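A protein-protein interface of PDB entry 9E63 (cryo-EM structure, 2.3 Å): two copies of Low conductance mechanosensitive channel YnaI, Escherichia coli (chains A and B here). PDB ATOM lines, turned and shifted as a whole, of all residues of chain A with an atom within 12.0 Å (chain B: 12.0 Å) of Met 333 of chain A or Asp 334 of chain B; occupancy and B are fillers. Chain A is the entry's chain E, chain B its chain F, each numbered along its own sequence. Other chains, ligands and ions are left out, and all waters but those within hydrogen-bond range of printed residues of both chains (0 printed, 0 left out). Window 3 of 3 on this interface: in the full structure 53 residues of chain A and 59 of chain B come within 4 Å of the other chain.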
ATOM      1  N   GLN A 329       4.601   8.183  22.970  1.00  0.00           N
ATOM      2  CA  GLN A 329       5.412   7.234  23.711  1.00  0.00           C
ATOM      3  C   GLN A 329       6.763   7.854  24.030  1.00  0.00           C
ATOM      4  O   GLN A 329       7.274   8.685  23.275  1.00  0.00           O
ATOM      5  CB  GLN A 329       5.623   5.938  22.925  1.00  0.00           C
ATOM      6  CG  GLN A 329       4.365   5.135  22.690  1.00  0.00           C
ATOM      7  CD  GLN A 329       4.630   3.655  22.616  1.00  0.00           C
ATOM      8  OE1 GLN A 329       4.642   3.072  21.536  1.00  0.00           O
ATOM      9  NE2 GLN A 329       4.844   3.033  23.766  1.00  0.00           N
ATOM     10  N   THR A 330       7.345   7.436  25.150  1.00  0.00           N
ATOM     11  CA  THR A 330       8.716   7.772  25.507  1.00  0.00           C
ATOM     12  C   THR A 330       9.558   6.516  25.359  1.00  0.00           C
ATOM     13  O   THR A 330       9.284   5.503  26.009  1.00  0.00           O
ATOM     14  CB  THR A 330       8.808   8.316  26.932  1.00  0.00           C
ATOM     15  OG1 THR A 330       8.113   9.565  27.014  1.00  0.00           O
ATOM     16  CG2 THR A 330      10.256   8.529  27.323  1.00  0.00           C
ATOM     17  N   LEU A 331      10.577   6.578  24.511  1.00  0.00           N
ATOM     18  CA  LEU A 331      11.378   5.415  24.160  1.00  0.00           C
ATOM     19  C   LEU A 331      12.785   5.562  24.720  1.00  0.00           C
ATOM     20  O   LEU A 331      13.417   6.607  24.555  1.00  0.00           O
ATOM     21  CB  LEU A 331      11.428   5.231  22.645  1.00  0.00           C
ATOM     22  CG  LEU A 331      10.073   5.131  21.948  1.00  0.00           C
ATOM     23  CD1 LEU A 331      10.258   4.914  20.464  1.00  0.00           C
ATOM     24  CD2 LEU A 331       9.248   4.014  22.553  1.00  0.00           C
ATOM     25  N   TYR A 332      13.265   4.513  25.382  1.00  0.00           N
ATOM     26  CA  TYR A 332      14.630   4.445  25.884  1.00  0.00           C
ATOM     27  C   TYR A 332      15.383   3.398  25.075  1.00  0.00           C
ATOM     28  O   TYR A 332      14.992   2.226  25.061  1.00  0.00           O
ATOM     29  CB  TYR A 332      14.651   4.093  27.370  1.00  0.00           C
ATOM     30  CG  TYR A 332      13.872   5.048  28.244  1.00  0.00           C
ATOM     31  CD1 TYR A 332      14.450   6.214  28.719  1.00  0.00           C
ATOM     32  CD2 TYR A 332      12.558   4.778  28.596  1.00  0.00           C
ATOM     33  CE1 TYR A 332      13.741   7.086  29.519  1.00  0.00           C
ATOM     34  CE2 TYR A 332      11.844   5.642  29.394  1.00  0.00           C
ATOM     35  CZ  TYR A 332      12.439   6.794  29.853  1.00  0.00           C
ATOM     36  OH  TYR A 332      11.727   7.658  30.648  1.00  0.00           O
ATOM     37  N   MET A 333      16.452   3.815  24.410  1.00  0.00           N
ATOM     38  CA  MET A 333      17.218   2.935  23.539  1.00  0.00           C
ATOM     39  C   MET A 333      18.577   2.631  24.152  1.00  0.00           C
ATOM     40  O   MET A 333      19.209   3.503  24.754  1.00  0.00           O
ATOM     41  CB  MET A 333      17.401   3.557  22.156  1.00  0.00           C
ATOM     42  CG  MET A 333      16.103   3.825  21.425  1.00  0.00           C
ATOM     43  SD  MET A 333      16.070   3.066  19.792  1.00  0.00           S
ATOM     44  CE  MET A 333      17.020   4.247  18.839  1.00  0.00           C
ATOM     45  N   ASP A 334      19.017   1.386  23.994  1.00  0.00           N
ATOM     46  CA  ASP A 334      20.301   0.935  24.523  1.00  0.00           C
ATOM     47  C   ASP A 334      21.467   1.736  23.951  1.00  0.00           C
ATOM     48  O   ASP A 334      22.247   2.339  24.691  1.00  0.00           O
ATOM     49  CB  ASP A 334      20.496  -0.551  24.233  1.00  0.00           C
ATOM     50  CG  ASP A 334      20.330  -0.885  22.762  1.00  0.00           C
ATOM     51  OD1 ASP A 334      19.953   0.014  21.981  1.00  0.00           O
ATOM     52  OD2 ASP A 334      20.577  -2.049  22.383  1.00  0.00           O
ATOM     53  N   THR B 330       3.580   9.944  18.099  1.00  0.00           N
ATOM     54  CA  THR B 330       4.629  10.907  18.405  1.00  0.00           C
ATOM     55  C   THR B 330       5.581  10.256  19.399  1.00  0.00           C
ATOM     56  O   THR B 330       5.156   9.816  20.469  1.00  0.00           O
ATOM     57  CB  THR B 330       4.054  12.201  18.978  1.00  0.00           C
ATOM     58  OG1 THR B 330       3.238  12.843  17.994  1.00  0.00           O
ATOM     59  CG2 THR B 330       5.167  13.143  19.385  1.00  0.00           C
ATOM     60  N   LEU B 331       6.860  10.194  19.048  1.00  0.00           N
ATOM     61  CA  LEU B 331       7.853   9.485  19.840  1.00  0.00           C
ATOM     62  C   LEU B 331       8.853  10.468  20.428  1.00  0.00           C
ATOM     63  O   LEU B 331       9.363  11.339  19.718  1.00  0.00           O
ATOM     64  CB  LEU B 331       8.578   8.440  18.992  1.00  0.00           C
ATOM     65  CG  LEU B 331       7.672   7.444  18.268  1.00  0.00           C
ATOM     66  CD1 LEU B 331       8.495   6.438  17.493  1.00  0.00           C
ATOM     67  CD2 LEU B 331       6.759   6.743  19.254  1.00  0.00           C
ATOM     68  N   TYR B 332       9.127  10.324  21.722  1.00  0.00           N
ATOM     69  CA  TYR B 332      10.117  11.133  22.423  1.00  0.00           C
ATOM     70  C   TYR B 332      11.276  10.235  22.831  1.00  0.00           C
ATOM     71  O   TYR B 332      11.080   9.262  23.561  1.00  0.00           O
ATOM     72  CB  TYR B 332       9.513  11.805  23.653  1.00  0.00           C
ATOM     73  CG  TYR B 332       8.334  12.691  23.351  1.00  0.00           C
ATOM     74  CD1 TYR B 332       8.516  14.001  22.941  1.00  0.00           C
ATOM     75  CD2 TYR B 332       7.039  12.220  23.485  1.00  0.00           C
ATOM     76  CE1 TYR B 332       7.443  14.813  22.663  1.00  0.00           C
ATOM     77  CE2 TYR B 332       5.959  13.026  23.212  1.00  0.00           C
ATOM     78  CZ  TYR B 332       6.168  14.322  22.803  1.00  0.00           C
ATOM     79  OH  TYR B 332       5.092  15.133  22.532  1.00  0.00           O
ATOM     80  N   MET B 333      12.473  10.568  22.369  1.00  0.00           N
ATOM     81  CA  MET B 333      13.656   9.763  22.626  1.00  0.00           C
ATOM     82  C   MET B 333      14.461  10.351  23.772  1.00  0.00           C
ATOM     83  O   MET B 333      14.424  11.562  24.017  1.00  0.00           O
ATOM     84  CB  MET B 333      14.526   9.670  21.377  1.00  0.00           C
ATOM     85  CG  MET B 333      13.735   9.376  20.134  1.00  0.00           C
ATOM     86  SD  MET B 333      13.606   7.618  19.789  1.00  0.00           S
ATOM     87  CE  MET B 333      15.252   7.089  20.233  1.00  0.00           C
ATOM     88  N   ASP B 334      15.183   9.487  24.476  1.00  0.00           N
ATOM     89  CA  ASP B 334      16.009   9.910  25.599  1.00  0.00           C
ATOM     90  C   ASP B 334      17.208  10.737  25.142  1.00  0.00           C
ATOM     91  O   ASP B 334      17.239  11.958  25.315  1.00  0.00           O
ATOM     92  CB  ASP B 334      16.483   8.692  26.389  1.00  0.00           C
ATOM     93  CG  ASP B 334      17.167   7.660  25.513  1.00  0.00           C
ATOM     94  OD1 ASP B 334      17.261   7.877  24.285  1.00  0.00           O
ATOM     95  OD2 ASP B 334      17.624   6.632  26.054  1.00  0.00           O
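The backbone NH of Gln 329 of chain A sits at hydrogen-bond distance from the backbone carbonyl oxygen of Thr 330 of chain B, at 3.0 Å. N of Tyr 332 of chain B sits at hydrogen-bond distance from O of Gln 329 of chain A (2.9 Å). The backbone NH (N) of Leu 331 of chain A sits at hydrogen-bond distance from the backbone carbonyl oxygen (O) of Tyr 332 of chain B. The backbone carbonyl oxygen of Leu 331 of chain A sits at hydrogen-bond distance from the backbone NH of Asp 334 of chain B, 3.4 Å away. N of Met 333 of chain A is in hydrogen-bond range of OD2 of Asp 334 of chain B.
Thr 330 of chain A touches Tyr 332 of chain B, but with the chains exchanged Tyr 332 of chain A does not touch Thr 330 of chain B (10.9 Å). Leu 331 of chain A touches Met 333 of chain B, but with the chains exchanged Met 333 of chain A does not touch Leu 331 of chain B (8.6 Å). Leu 331 of chain A touches Asp 334 of chain B, but with the chains exchanged Asp 334 of chain A does not touch Leu 331 of chain B (13.4 Å). Met 333 of chain B touches its own counterpart, Met 333 of chain A. Positions printed for both chains: 330, 331, 332, 333 and 334. Of the 11 pairs that touch across the chains among the printed residues, 2 have their exchanged pair printed and touching as well.
Of the 5 printed residues of chain B, 5 touch a printed residue of chain A. Hydrophobic or aromatic side chains of chain B within 4 Å of the printed part of chain A: Leu 331, Tyr 332 and Met 333. Of the 6 printed residues of chain A, 5 touch a printed residue of chain B. Printed residues of chain A that touch a printed residue of chain B: Gln 329, Thr 330, Leu 331, Tyr 332 and Met 333. Among the printed residues, 11 pairs touch across the chains.
Among the printed residues, merely in contact across the chains: Gln 329 of chain A with Leu 331 of chain B, Thr 330 of chain A with Tyr 332 of chain B, Leu 331 of chain A with Leu 331 of chain B, Leu 331 of chain A with Met 333 of chain B, Tyr 332 of chain A with Asp 334 of chain B and Met 333 of chain A with Met 333 of chain B.
Of chain B, only Met 333 (3.6 Å) and Asp 334 (3.5 Å) come within 4 Å of Met 333 of chain A. Asp 334 of chain B touches just these residues of chain A: Leu 331 (3.4 Å), Tyr 332 (3.7 Å) and Met 333 (3.5 Å). Leu 331 of chain A touches just these residues of chain B: Leu 331 (3.8 Å), Tyr 332 (2.9 Å), Met 333 (3.7 Å) and Asp 334 (3.4 Å). No residue of chain B comes within 4 Å of Asp 334 of chain A. Of chain A, only Leu 331 and Met 333 come within 4 Å of Met 333 of chain B. Of the printed residues of chain A, Thr 330 of chain B touches Gln 329. Of the printed residues of chain B, Thr 330 of chain A touches Tyr 332. Printed residues of chain B within 4 Å of Gln 329 of chain A: Thr 330 (3.0 Å), Leu 331 (3.6 Å) and Tyr 332 (2.9 Å). Of the printed residues of chain A, Leu 331 of chain B touches Gln 329 and Leu 331. Of the printed residues of chain A, Tyr 332 of chain B touches Gln 329, Thr 330 and Leu 331. The nearest residue of chain B that does not touch Met 333 of chain A is Tyr 332 of chain B (7.7 Å).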
